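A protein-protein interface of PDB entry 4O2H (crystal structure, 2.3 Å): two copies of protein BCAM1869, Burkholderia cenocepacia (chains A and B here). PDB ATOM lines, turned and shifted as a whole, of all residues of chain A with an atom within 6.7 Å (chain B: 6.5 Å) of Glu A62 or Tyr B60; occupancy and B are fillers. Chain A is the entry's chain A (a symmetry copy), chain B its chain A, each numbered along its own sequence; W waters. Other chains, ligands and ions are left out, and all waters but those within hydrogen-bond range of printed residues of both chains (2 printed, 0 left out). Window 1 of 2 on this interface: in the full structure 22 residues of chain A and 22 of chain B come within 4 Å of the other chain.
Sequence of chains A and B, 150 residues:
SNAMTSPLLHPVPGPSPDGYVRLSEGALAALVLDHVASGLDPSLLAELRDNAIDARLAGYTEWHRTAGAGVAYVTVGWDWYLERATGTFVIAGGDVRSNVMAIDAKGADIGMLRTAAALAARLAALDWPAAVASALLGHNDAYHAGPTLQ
OD2 of Asp B41 is in salt-bridge range of NE of Arg A97.
A ring nitrogen (ND1) of His B139 sits close to the side-chain hydroxyl (OH) of Tyr A73, at 3.3 Å.
O of Ala B37 lies close to OG1 of Thr B61.
The backbone NH of Glu B62 is in hydrogen-bond range of the backbone carbonyl oxygen of Ala B37, at 2.7 Å.
The backbone NH of Asp B41 is in hydrogen-bond range of the backbone carbonyl oxygen of Ala B58, 2.8 Å away.
N of Val A36 lies within hydrogen-bond range of O of Glu A62, 2.8 Å away.
OH of Tyr A73 is in hydrogen-bond range of ND1 of His A64, at 2.7 Å.
The backbone carbonyl oxygen of Arg A97 lies within hydrogen-bond range of the backbone NH of Gly A77.
Ala B37 touches Val A36 (CB to CG1, 3.9 Å).
Glu B62 touches Tyr A60.
Arg B97 touches Tyr A60 (NH2 to CD2, 3.4 Å).
CZ of Tyr B60 touches OE1 of Glu A62, 3.5 Å away.
Thr A75 touches Leu B40 (OG1 to O, 3.8 Å).
NH2 of Arg A97 touches CD2 of Tyr B60, 3.4 Å away.
Printed residues of chain B within 4 Å of Val A36: Ala B37 (3.9 Å).
Glu A62 touches one residue of chain B.
Of the printed residues of chain B, Arg A97 touches Asp B41 and Tyr B60.
Printed residues of chain A within 4 Å of Ala B37: Val A36 (3.9 Å).
Of the printed residues of chain A, Leu B40 touches Thr A75.
Of chain A, only Glu A62 (3.5 Å) and Arg A97 (3.4 Å) come within 4 Å of Tyr B60.
Of the printed residues of chain A, Glu B62 touches Tyr A60.
Asp B79 touches none of the printed residues of chain A.
The nearest printed residue of chain A that does not touch Arg B97 is Glu A62 (6.4 Å).
Of the 17 printed residues of chain A, 6 touch a printed residue of chain B.
Printed residues of chain A that touch a printed residue of chain B: Val A36, Tyr A60, Glu A62, Tyr A73, Thr A75 and Arg A97.
Along chain A the printed residues that touch a printed residue of chain B span positions 36 to 97.
Among the printed residues, Asp or Glu carboxylates within 4 Å of a Lys or Arg side-chain nitrogen of the other chain: Arg A97 with Asp B41.
Tyr A60 touches Glu B62, and with the chains exchanged Glu A62 touches Tyr B60.
Tyr A60 touches Arg B97, and with the chains exchanged Arg A97 touches Tyr B60.
Positions printed for both chains: 37, 38, 60, 61, 62, 78, 97 and 132.
Of the 8 pairs that touch across the chains among the printed residues, 4 have their exchanged pair printed and touching as well.
Water W1 lies within hydrogen-bond range of O of Leu B40, OG1 of Thr A75 and NH1 of Arg A97.
Water W2 lies within hydrogen-bond range of OE2 of Glu B62 (2.7 Å) and OE2 of Glu A62 (2.7 Å).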
ATOM      1  N   ASP A  34     -15.129  34.722 -19.039  1.00  0.00           N
ATOM      2  CA  ASP A  34     -13.929  33.919 -18.891  1.00  0.00           C
ATOM      3  C   ASP A  34     -14.015  32.733 -19.803  1.00  0.00           C
ATOM      4  O   ASP A  34     -15.108  32.205 -20.005  1.00  0.00           O
ATOM      5  CB  ASP A  34     -13.782  33.437 -17.439  1.00  0.00           C
ATOM      6  CG  ASP A  34     -13.743  34.552 -16.419  1.00  0.00           C
ATOM      7  OD1 ASP A  34     -13.015  35.548 -16.652  1.00  0.00           O
ATOM      8  OD2 ASP A  34     -14.432  34.421 -15.371  1.00  0.00           O
ATOM      9  N   HIS A  35     -12.880  32.334 -20.380  1.00  0.00           N
ATOM     10  CA  HIS A  35     -12.775  31.163 -21.246  1.00  0.00           C
ATOM     11  C   HIS A  35     -12.938  29.912 -20.388  1.00  0.00           C
ATOM     12  O   HIS A  35     -12.333  29.817 -19.333  1.00  0.00           O
ATOM     13  CB  HIS A  35     -11.423  31.137 -22.003  1.00  0.00           C
ATOM     14  CG  HIS A  35     -11.136  29.822 -22.676  1.00  0.00           C
ATOM     15  ND1 HIS A  35     -10.545  28.772 -21.990  1.00  0.00           N
ATOM     16  CD2 HIS A  35     -11.443  29.403 -23.925  1.00  0.00           C
ATOM     17  CE1 HIS A  35     -10.475  27.774 -22.851  1.00  0.00           C
ATOM     18  NE2 HIS A  35     -10.984  28.111 -24.031  1.00  0.00           N
ATOM     19  N   VAL A  36     -13.702  28.936 -20.880  1.00  0.00           N
ATOM     20  CA  VAL A  36     -13.971  27.670 -20.184  1.00  0.00           C
ATOM     21  C   VAL A  36     -13.364  26.544 -21.011  1.00  0.00           C
ATOM     22  O   VAL A  36     -12.619  25.737 -20.472  1.00  0.00           O
ATOM     23  CB  VAL A  36     -15.497  27.475 -19.954  1.00  0.00           C
ATOM     24  CG1 VAL A  36     -15.810  26.177 -19.218  1.00  0.00           C
ATOM     25  CG2 VAL A  36     -16.117  28.668 -19.209  1.00  0.00           C
ATOM     26  N   ALA A  37     -13.684  26.472 -22.316  1.00  0.00           N
ATOM     27  CA  ALA A  37     -13.182  25.380 -23.150  1.00  0.00           C
ATOM     28  C   ALA A  37     -13.226  25.736 -24.605  1.00  0.00           C
ATOM     29  O   ALA A  37     -14.042  26.518 -25.045  1.00  0.00           O
ATOM     30  CB  ALA A  37     -13.976  24.082 -22.898  1.00  0.00           C
ATOM     31  N   SER A  38     -12.293  25.175 -25.345  1.00  0.00           N
ATOM     32  CA  SER A  38     -12.124  25.334 -26.779  1.00  0.00           C
ATOM     33  C   SER A  38     -11.629  24.004 -27.319  1.00  0.00           C
ATOM     34  O   SER A  38     -10.955  23.267 -26.611  1.00  0.00           O
ATOM     35  CB  SER A  38     -11.142  26.461 -27.084  1.00  0.00           C
ATOM     36  OG  SER A  38     -11.596  27.738 -26.660  1.00  0.00           O
ATOM     37  N   TYR A  60     -14.983  24.962 -31.738  1.00  0.00           N
ATOM     38  CA  TYR A  60     -15.901  25.488 -30.760  1.00  0.00           C
ATOM     39  C   TYR A  60     -15.115  26.170 -29.634  1.00  0.00           C
ATOM     40  O   TYR A  60     -13.916  25.934 -29.440  1.00  0.00           O
ATOM     41  CB  TYR A  60     -16.798  24.343 -30.208  1.00  0.00           C
ATOM     42  CG  TYR A  60     -16.118  23.495 -29.147  1.00  0.00           C
ATOM     43  CD1 TYR A  60     -16.134  23.874 -27.805  1.00  0.00           C
ATOM     44  CD2 TYR A  60     -15.427  22.329 -29.490  1.00  0.00           C
ATOM     45  CE1 TYR A  60     -15.465  23.130 -26.832  1.00  0.00           C
ATOM     46  CE2 TYR A  60     -14.791  21.553 -28.515  1.00  0.00           C
ATOM     47  CZ  TYR A  60     -14.780  21.983 -27.195  1.00  0.00           C
ATOM     48  OH  TYR A  60     -14.129  21.267 -26.219  1.00  0.00           O
ATOM     49  N   THR A  61     -15.814  27.019 -28.904  1.00  0.00           N
ATOM     50  CA  THR A  61     -15.332  27.674 -27.699  1.00  0.00           C
ATOM     51  C   THR A  61     -16.554  27.975 -26.835  1.00  0.00           C
ATOM     52  O   THR A  61     -17.634  28.211 -27.363  1.00  0.00           O
ATOM     53  CB  THR A  61     -14.434  28.861 -27.983  1.00  0.00           C
ATOM     54  OG1 THR A  61     -13.884  29.295 -26.738  1.00  0.00           O
ATOM     55  CG2 THR A  61     -15.150  29.981 -28.721  1.00  0.00           C
ATOM     56  N   GLU A  62     -16.367  27.832 -25.518  1.00  0.00           N
ATOM     57  CA  GLU A  62     -17.316  28.027 -24.430  1.00  0.00           C
ATOM     58  C   GLU A  62     -16.729  28.980 -23.390  1.00  0.00           C
ATOM     59  O   GLU A  62     -15.604  28.787 -22.953  1.00  0.00           O
ATOM     60  CB  GLU A  62     -17.698  26.679 -23.773  1.00  0.00           C
ATOM     61  CG  GLU A  62     -18.613  25.835 -24.646  1.00  0.00           C
ATOM     62  CD  GLU A  62     -19.899  26.497 -25.132  1.00  0.00           C
ATOM     63  OE1 GLU A  62     -20.389  27.476 -24.516  1.00  0.00           O
ATOM     64  OE2 GLU A  62     -20.444  25.976 -26.127  1.00  0.00           O
ATOM     65  N   TRP A  63     -17.492  30.029 -23.050  1.00  0.00           N
ATOM     66  CA  TRP A  63     -17.124  31.111 -22.140  1.00  0.00           C
ATOM     67  C   TRP A  63     -18.255  31.300 -21.127  1.00  0.00           C
ATOM     68  O   TRP A  63     -19.392  30.895 -21.381  1.00  0.00           O
ATOM     69  CB  TRP A  63     -16.860  32.428 -22.948  1.00  0.00           C
ATOM     70  CG  TRP A  63     -15.596  32.401 -23.792  1.00  0.00           C
ATOM     71  CD1 TRP A  63     -15.251  31.472 -24.732  1.00  0.00           C
ATOM     72  CD2 TRP A  63     -14.464  33.280 -23.660  1.00  0.00           C
ATOM     73  NE1 TRP A  63     -13.991  31.727 -25.213  1.00  0.00           N
ATOM     74  CE2 TRP A  63     -13.485  32.841 -24.576  1.00  0.00           C
ATOM     75  CE3 TRP A  63     -14.208  34.434 -22.892  1.00  0.00           C
ATOM     76  CZ2 TRP A  63     -12.273  33.532 -24.773  1.00  0.00           C
ATOM     77  CZ3 TRP A  63     -12.987  35.100 -23.055  1.00  0.00           C
ATOM     78  CH2 TRP A  63     -12.026  34.634 -23.966  1.00  0.00           C
ATOM     79  N   HIS A  64     -17.936  31.829 -19.951  1.00  0.00           N
ATOM     80  CA  HIS A  64     -18.985  32.013 -18.950  1.00  0.00           C
ATOM     81  C   HIS A  64     -18.645  33.159 -17.991  1.00  0.00           C
ATOM     82  O   HIS A  64     -17.504  33.616 -17.902  1.00  0.00           O
ATOM     83  CB  HIS A  64     -19.327  30.679 -18.190  1.00  0.00           C
ATOM     84  CG  HIS A  64     -18.339  30.195 -17.149  1.00  0.00           C
ATOM     85  ND1 HIS A  64     -18.559  28.999 -16.448  1.00  0.00           N
ATOM     86  CD2 HIS A  64     -17.162  30.732 -16.723  1.00  0.00           C
ATOM     87  CE1 HIS A  64     -17.515  28.851 -15.643  1.00  0.00           C
ATOM     88  NE2 HIS A  64     -16.652  29.871 -15.759  1.00  0.00           N
ATOM     89  N   TYR A  73     -25.586  33.709 -13.736  1.00  0.00           N
ATOM     90  CA  TYR A  73     -24.657  32.885 -14.486  1.00  0.00           C
ATOM     91  C   TYR A  73     -24.926  33.107 -15.968  1.00  0.00           C
ATOM     92  O   TYR A  73     -26.073  33.031 -16.386  1.00  0.00           O
ATOM     93  CB  TYR A  73     -24.788  31.410 -14.096  1.00  0.00           C
ATOM     94  CG  TYR A  73     -23.803  30.510 -14.819  1.00  0.00           C
ATOM     95  CD1 TYR A  73     -22.442  30.546 -14.516  1.00  0.00           C
ATOM     96  CD2 TYR A  73     -24.233  29.610 -15.796  1.00  0.00           C
ATOM     97  CE1 TYR A  73     -21.534  29.712 -15.160  1.00  0.00           C
ATOM     98  CE2 TYR A  73     -23.322  28.797 -16.479  1.00  0.00           C
ATOM     99  CZ  TYR A  73     -21.979  28.841 -16.143  1.00  0.00           C
ATOM    100  OH  TYR A  73     -21.087  28.033 -16.785  1.00  0.00           O
ATOM    101  N   THR A  75     -23.649  32.102 -19.991  1.00  0.00           N
ATOM    102  CA  THR A  75     -22.909  31.202 -20.920  1.00  0.00           C
ATOM    103  C   THR A  75     -22.931  31.776 -22.323  1.00  0.00           C
ATOM    104  O   THR A  75     -23.957  32.276 -22.779  1.00  0.00           O
ATOM    105  CB  THR A  75     -23.529  29.809 -21.002  1.00  0.00           C
ATOM    106  OG1 THR A  75     -24.940  29.971 -21.096  1.00  0.00           O
ATOM    107  CG2 THR A  75     -23.193  28.967 -19.830  1.00  0.00           C
ATOM    108  N   VAL A  76     -21.811  31.733 -22.987  1.00  0.00           N
ATOM    109  CA  VAL A  76     -21.629  32.249 -24.333  1.00  0.00           C
ATOM    110  C   VAL A  76     -20.684  31.297 -25.038  1.00  0.00           C
ATOM    111  O   VAL A  76     -19.553  31.061 -24.572  1.00  0.00           O
ATOM    112  CB  VAL A  76     -21.095  33.723 -24.346  1.00  0.00           C
ATOM    113  CG1 VAL A  76     -20.981  34.273 -25.780  1.00  0.00           C
ATOM    114  CG2 VAL A  76     -21.954  34.650 -23.459  1.00  0.00           C
ATOM    115  N   GLY A  77     -21.170  30.739 -26.135  1.00  0.00           N
ATOM    116  CA  GLY A  77     -20.407  29.813 -26.955  1.00  0.00           C
ATOM    117  C   GLY A  77     -20.585  30.105 -28.418  1.00  0.00           C
ATOM    118  O   GLY A  77     -21.558  30.732 -28.822  1.00  0.00           O
ATOM    119  N   TRP A  78     -19.611  29.731 -29.209  1.00  0.00           N
ATOM    120  CA  TRP A  78     -19.662  29.965 -30.642  1.00  0.00           C
ATOM    121  C   TRP A  78     -18.670  29.058 -31.345  1.00  0.00           C
ATOM    122  O   TRP A  78     -17.761  28.479 -30.716  1.00  0.00           O
ATOM    123  CB  TRP A  78     -19.373  31.462 -30.985  1.00  0.00           C
ATOM    124  CG  TRP A  78     -17.975  31.921 -30.629  1.00  0.00           C
ATOM    125  CD1 TRP A  78     -16.913  32.059 -31.488  1.00  0.00           C
ATOM    126  CD2 TRP A  78     -17.538  32.455 -29.360  1.00  0.00           C
ATOM    127  NE1 TRP A  78     -15.839  32.601 -30.829  1.00  0.00           N
ATOM    128  CE2 TRP A  78     -16.190  32.858 -29.521  1.00  0.00           C
ATOM    129  CE3 TRP A  78     -18.141  32.585 -28.092  1.00  0.00           C
ATOM    130  CZ2 TRP A  78     -15.428  33.370 -28.456  1.00  0.00           C
ATOM    131  CZ3 TRP A  78     -17.379  33.058 -27.036  1.00  0.00           C
ATOM    132  CH2 TRP A  78     -16.047  33.472 -27.225  1.00  0.00           C
ATOM    133  N   ARG A  97     -24.089  31.611 -29.478  1.00  0.00           N
ATOM    134  CA  ARG A  97     -25.082  30.951 -28.663  1.00  0.00           C
ATOM    135  C   ARG A  97     -24.854  31.359 -27.218  1.00  0.00           C
ATOM    136  O   ARG A  97     -23.725  31.309 -26.746  1.00  0.00           O
ATOM    137  CB  ARG A  97     -25.042  29.428 -28.849  1.00  0.00           C
ATOM    138  CG  ARG A  97     -26.211  28.696 -28.168  1.00  0.00           C
ATOM    139  CD  ARG A  97     -25.859  28.109 -26.800  1.00  0.00           C
ATOM    140  NE  ARG A  97     -24.811  27.109 -26.957  1.00  0.00           N
ATOM    141  CZ  ARG A  97     -23.622  27.141 -26.368  1.00  0.00           C
ATOM    142  NH1 ARG A  97     -23.339  28.088 -25.458  1.00  0.00           N
ATOM    143  NH2 ARG A  97     -22.732  26.194 -26.621  1.00  0.00           N
ATOM    144  N   VAL A 132      -8.532  31.390 -26.867  1.00  0.00           N
ATOM    145  CA  VAL A 132      -8.836  30.204 -27.671  1.00  0.00           C
ATOM    146  C   VAL A 132      -7.527  29.535 -28.141  1.00  0.00           C
ATOM    147  O   VAL A 132      -7.339  28.337 -27.897  1.00  0.00           O
ATOM    148  CB  VAL A 132      -9.776  30.551 -28.850  1.00  0.00           C
ATOM    149  CG1 VAL A 132      -9.853  29.432 -29.902  1.00  0.00           C
ATOM    150  CG2 VAL A 132     -11.160  30.926 -28.326  1.00  0.00           C
ATOM    151  N   ALA B  37     -17.524  20.640 -19.630  1.00  0.00           N
ATOM    152  CA  ALA B  37     -18.476  21.734 -19.436  1.00  0.00           C
ATOM    153  C   ALA B  37     -19.832  21.383 -19.970  1.00  0.00           C
ATOM    154  O   ALA B  37     -19.972  20.606 -20.890  1.00  0.00           O
ATOM    155  CB  ALA B  37     -17.967  23.032 -20.094  1.00  0.00           C
ATOM    156  N   SER B  38     -20.841  21.945 -19.340  1.00  0.00           N
ATOM    157  CA  SER B  38     -22.249  21.791 -19.666  1.00  0.00           C
ATOM    158  C   SER B  38     -22.921  23.121 -19.377  1.00  0.00           C
ATOM    159  O   SER B  38     -22.480  23.854 -18.501  1.00  0.00           O
ATOM    160  CB  SER B  38     -22.870  20.662 -18.849  1.00  0.00           C
ATOM    161  OG  SER B  38     -22.322  19.385 -19.137  1.00  0.00           O
ATOM    162  N   GLY B  39     -23.944  23.443 -20.137  1.00  0.00           N
ATOM    163  CA  GLY B  39     -24.709  24.659 -19.937  1.00  0.00           C
ATOM    164  C   GLY B  39     -26.059  24.568 -20.587  1.00  0.00           C
ATOM    165  O   GLY B  39     -26.324  23.657 -21.374  1.00  0.00           O
ATOM    166  N   LEU B  40     -26.933  25.491 -20.216  1.00  0.00           N
ATOM    167  CA  LEU B  40     -28.279  25.557 -20.750  1.00  0.00           C
ATOM    168  C   LEU B  40     -28.297  26.391 -22.025  1.00  0.00           C
ATOM    169  O   LEU B  40     -27.519  27.338 -22.143  1.00  0.00           O
ATOM    170  CB  LEU B  40     -29.240  26.163 -19.695  1.00  0.00           C
ATOM    171  CG  LEU B  40     -29.336  25.372 -18.368  1.00  0.00           C
ATOM    172  CD1 LEU B  40     -30.382  25.992 -17.442  1.00  0.00           C
ATOM    173  CD2 LEU B  40     -29.593  23.847 -18.600  1.00  0.00           C
ATOM    174  N   ASP B  41     -29.131  25.988 -23.007  1.00  0.00           N
ATOM    175  CA  ASP B  41     -29.351  26.752 -24.252  1.00  0.00           C
ATOM    176  C   ASP B  41     -30.877  27.051 -24.365  1.00  0.00           C
ATOM    177  O   ASP B  41     -31.605  26.214 -24.899  1.00  0.00           O
ATOM    178  CB  ASP B  41     -28.793  26.010 -25.510  1.00  0.00           C
ATOM    179  CG  ASP B  41     -28.932  26.787 -26.819  1.00  0.00           C
ATOM    180  OD1 ASP B  41     -29.462  27.910 -26.792  1.00  0.00           O
ATOM    181  OD2 ASP B  41     -28.411  26.315 -27.849  1.00  0.00           O
ATOM    182  N   LEU B  44     -32.286  26.641 -27.942  1.00  0.00           N
ATOM    183  CA  LEU B  44     -32.468  25.244 -28.325  1.00  0.00           C
ATOM    184  C   LEU B  44     -33.742  24.677 -27.677  1.00  0.00           C
ATOM    185  O   LEU B  44     -34.524  24.009 -28.363  1.00  0.00           O
ATOM    186  CB  LEU B  44     -31.250  24.397 -27.938  1.00  0.00           C
ATOM    187  CG  LEU B  44     -31.359  22.851 -28.155  1.00  0.00           C
ATOM    188  CD1 LEU B  44     -31.557  22.500 -29.624  1.00  0.00           C
ATOM    189  CD2 LEU B  44     -30.136  22.141 -27.612  1.00  0.00           C
ATOM    190  N   ALA B  58     -32.712  22.117 -22.013  1.00  0.00           N
ATOM    191  CA  ALA B  58     -31.894  21.750 -23.138  1.00  0.00           C
ATOM    192  C   ALA B  58     -30.589  22.486 -23.047  1.00  0.00           C
ATOM    193  O   ALA B  58     -30.540  23.613 -22.540  1.00  0.00           O
ATOM    194  CB  ALA B  58     -32.599  22.070 -24.443  1.00  0.00           C
ATOM    195  N   GLY B  59     -29.538  21.883 -23.586  1.00  0.00           N
ATOM    196  CA  GLY B  59     -28.243  22.537 -23.570  1.00  0.00           C
ATOM    197  C   GLY B  59     -27.177  21.759 -24.280  1.00  0.00           C
ATOM    198  O   GLY B  59     -27.453  20.780 -24.981  1.00  0.00           O
ATOM    199  N   TYR B  60     -25.950  22.189 -24.030  1.00  0.00           N
ATOM    200  CA  TYR B  60     -24.720  21.661 -24.566  1.00  0.00           C
ATOM    201  C   TYR B  60     -23.927  20.973 -23.448  1.00  0.00           C
ATOM    202  O   TYR B  60     -24.150  21.205 -22.254  1.00  0.00           O
ATOM    203  CB  TYR B  60     -23.895  22.807 -25.219  1.00  0.00           C
ATOM    204  CG  TYR B  60     -23.124  23.649 -24.219  1.00  0.00           C
ATOM    205  CD1 TYR B  60     -21.856  23.265 -23.781  1.00  0.00           C
ATOM    206  CD2 TYR B  60     -23.676  24.814 -23.679  1.00  0.00           C
ATOM    207  CE1 TYR B  60     -21.165  24.003 -22.819  1.00  0.00           C
ATOM    208  CE2 TYR B  60     -22.971  25.585 -22.747  1.00  0.00           C
ATOM    209  CZ  TYR B  60     -21.733  25.150 -22.293  1.00  0.00           C
ATOM    210  OH  TYR B  60     -21.033  25.860 -21.348  1.00  0.00           O
ATOM    211  N   THR B  61     -23.006  20.124 -23.863  1.00  0.00           N
ATOM    212  CA  THR B  61     -22.038  19.463 -23.005  1.00  0.00           C
ATOM    213  C   THR B  61     -20.812  19.162 -23.865  1.00  0.00           C
ATOM    214  O   THR B  61     -20.944  18.930 -25.060  1.00  0.00           O
ATOM    215  CB  THR B  61     -22.611  18.274 -22.261  1.00  0.00           C
ATOM    216  OG1 THR B  61     -21.626  17.834 -21.323  1.00  0.00           O
ATOM    217  CG2 THR B  61     -23.066  17.159 -23.188  1.00  0.00           C
ATOM    218  N   GLU B  62     -19.635  19.299 -23.243  1.00  0.00           N
ATOM    219  CA  GLU B  62     -18.291  19.103 -23.769  1.00  0.00           C
ATOM    220  C   GLU B  62     -17.513  18.144 -22.869  1.00  0.00           C
ATOM    221  O   GLU B  62     -17.481  18.332 -21.661  1.00  0.00           O
ATOM    222  CB  GLU B  62     -17.540  20.449 -23.902  1.00  0.00           C
ATOM    223  CG  GLU B  62     -18.051  21.298 -25.055  1.00  0.00           C
ATOM    224  CD  GLU B  62     -18.075  20.642 -26.432  1.00  0.00           C
ATOM    225  OE1 GLU B  62     -17.332  19.662 -26.689  1.00  0.00           O
ATOM    226  OE2 GLU B  62     -18.826  21.168 -27.279  1.00  0.00           O
ATOM    227  N   TRP B  78     -22.018  17.422 -27.549  1.00  0.00           N
ATOM    228  CA  TRP B  78     -23.351  17.194 -28.083  1.00  0.00           C
ATOM    229  C   TRP B  78     -24.346  18.101 -27.383  1.00  0.00           C
ATOM    230  O   TRP B  78     -24.059  18.675 -26.313  1.00  0.00           O
ATOM    231  CB  TRP B  78     -23.775  15.697 -27.932  1.00  0.00           C
ATOM    232  CG  TRP B  78     -23.913  15.234 -26.499  1.00  0.00           C
ATOM    233  CD1 TRP B  78     -25.082  15.096 -25.789  1.00  0.00           C
ATOM    234  CD2 TRP B  78     -22.869  14.694 -25.660  1.00  0.00           C
ATOM    235  NE1 TRP B  78     -24.826  14.549 -24.557  1.00  0.00           N
ATOM    236  CE2 TRP B  78     -23.477  14.287 -24.447  1.00  0.00           C
ATOM    237  CE3 TRP B  78     -21.471  14.560 -25.800  1.00  0.00           C
ATOM    238  CZ2 TRP B  78     -22.733  13.770 -23.372  1.00  0.00           C
ATOM    239  CZ3 TRP B  78     -20.736  14.082 -24.728  1.00  0.00           C
ATOM    240  CH2 TRP B  78     -21.365  13.665 -23.540  1.00  0.00           C
ATOM    241  N   ASP B  79     -25.526  18.203 -27.994  1.00  0.00           N
ATOM    242  CA  ASP B  79     -26.710  18.862 -27.444  1.00  0.00           C
ATOM    243  C   ASP B  79     -27.572  17.820 -26.782  1.00  0.00           C
ATOM    244  O   ASP B  79     -27.697  16.682 -27.276  1.00  0.00           O
ATOM    245  CB  ASP B  79     -27.506  19.623 -28.523  1.00  0.00           C
ATOM    246  CG  ASP B  79     -26.829  20.871 -29.053  1.00  0.00           C
ATOM    247  OD1 ASP B  79     -25.822  21.315 -28.444  1.00  0.00           O
ATOM    248  OD2 ASP B  79     -27.313  21.419 -30.056  1.00  0.00           O
ATOM    249  N   TRP B  80     -28.146  18.189 -25.635  1.00  0.00           N
ATOM    250  CA  TRP B  80     -29.019  17.281 -24.876  1.00  0.00           C
ATOM    251  C   TRP B  80     -30.320  17.984 -24.491  1.00  0.00           C
ATOM    252  O   TRP B  80     -30.417  19.190 -24.572  1.00  0.00           O
ATOM    253  CB  TRP B  80     -28.304  16.749 -23.612  1.00  0.00           C
ATOM    254  CG  TRP B  80     -27.825  17.871 -22.730  1.00  0.00           C
ATOM    255  CD1 TRP B  80     -26.595  18.460 -22.761  1.00  0.00           C
ATOM    256  CD2 TRP B  80     -28.613  18.633 -21.793  1.00  0.00           C
ATOM    257  NE1 TRP B  80     -26.561  19.528 -21.901  1.00  0.00           N
ATOM    258  CE2 TRP B  80     -27.789  19.663 -21.298  1.00  0.00           C
ATOM    259  CE3 TRP B  80     -29.937  18.527 -21.304  1.00  0.00           C
ATOM    260  CZ2 TRP B  80     -28.252  20.611 -20.372  1.00  0.00           C
ATOM    261  CZ3 TRP B  80     -30.391  19.463 -20.387  1.00  0.00           C
ATOM    262  CH2 TRP B  80     -29.554  20.485 -19.923  1.00  0.00           C
ATOM    263  N   ARG B  97     -20.764  15.555 -31.862  1.00  0.00           N
ATOM    264  CA  ARG B  97     -19.660  16.215 -32.520  1.00  0.00           C
ATOM    265  C   ARG B  97     -18.378  15.801 -31.818  1.00  0.00           C
ATOM    266  O   ARG B  97     -18.314  15.846 -30.596  1.00  0.00           O
ATOM    267  CB  ARG B  97     -19.844  17.739 -32.539  1.00  0.00           C
ATOM    268  CG  ARG B  97     -18.806  18.471 -33.406  1.00  0.00           C
ATOM    269  CD  ARG B  97     -17.637  19.052 -32.611  1.00  0.00           C
ATOM    270  NE  ARG B  97     -18.135  20.050 -31.673  1.00  0.00           N
ATOM    271  CZ  ARG B  97     -17.982  20.013 -30.356  1.00  0.00           C
ATOM    272  NH1 ARG B  97     -17.225  19.061 -29.787  1.00  0.00           N
ATOM    273  NH2 ARG B  97     -18.520  20.958 -29.600  1.00  0.00           N
ATOM    274  N   VAL B 132     -23.562  15.726 -16.338  1.00  0.00           N
ATOM    275  CA  VAL B 132     -24.212  16.916 -16.891  1.00  0.00           C
ATOM    276  C   VAL B 132     -25.094  17.583 -15.815  1.00  0.00           C
ATOM    277  O   VAL B 132     -24.925  18.779 -15.550  1.00  0.00           O
ATOM    278  CB  VAL B 132     -25.006  16.575 -18.175  1.00  0.00           C
ATOM    279  CG1 VAL B 132     -25.966  17.698 -18.599  1.00  0.00           C
ATOM    280  CG2 VAL B 132     -24.045  16.201 -19.302  1.00  0.00           C
ATOM    281  N   LEU B 136     -24.643  21.306 -14.017  1.00  0.00           N
ATOM    282  CA  LEU B 136     -25.762  22.251 -14.094  1.00  0.00           C
ATOM    283  C   LEU B 136     -26.129  22.787 -12.719  1.00  0.00           C
ATOM    284  O   LEU B 136     -26.506  23.958 -12.607  1.00  0.00           O
ATOM    285  CB  LEU B 136     -26.990  21.591 -14.731  1.00  0.00           C
ATOM    286  CG  LEU B 136     -26.894  21.231 -16.210  1.00  0.00           C
ATOM    287  CD1 LEU B 136     -28.207  20.720 -16.676  1.00  0.00           C
ATOM    288  CD2 LEU B 136     -26.439  22.428 -17.085  1.00  0.00           C
ATOM    289  N   HIS B 139     -23.326  25.448 -11.425  1.00  0.00           N
ATOM    290  CA  HIS B 139     -23.422  26.785 -12.024  1.00  0.00           C
ATOM    291  C   HIS B 139     -24.262  27.772 -11.215  1.00  0.00           C
ATOM    292  O   HIS B 139     -24.039  28.972 -11.314  1.00  0.00           O
ATOM    293  CB  HIS B 139     -24.007  26.680 -13.431  1.00  0.00           C
ATOM    294  CG  HIS B 139     -23.088  25.998 -14.385  1.00  0.00           C
ATOM    295  ND1 HIS B 139     -21.710  26.055 -14.225  1.00  0.00           N
ATOM    296  CD2 HIS B 139     -23.373  25.275 -15.491  1.00  0.00           C
ATOM    297  CE1 HIS B 139     -21.206  25.367 -15.231  1.00  0.00           C
ATOM    298  NE2 HIS B 139     -22.166  24.879 -16.020  1.00  0.00           N
HETATM  299  O   HOH W   1     -25.782  28.880 -23.530  1.00  0.00           O
HETATM  300  O   HOH W   2     -20.128  23.573 -27.403  1.00  0.00           O
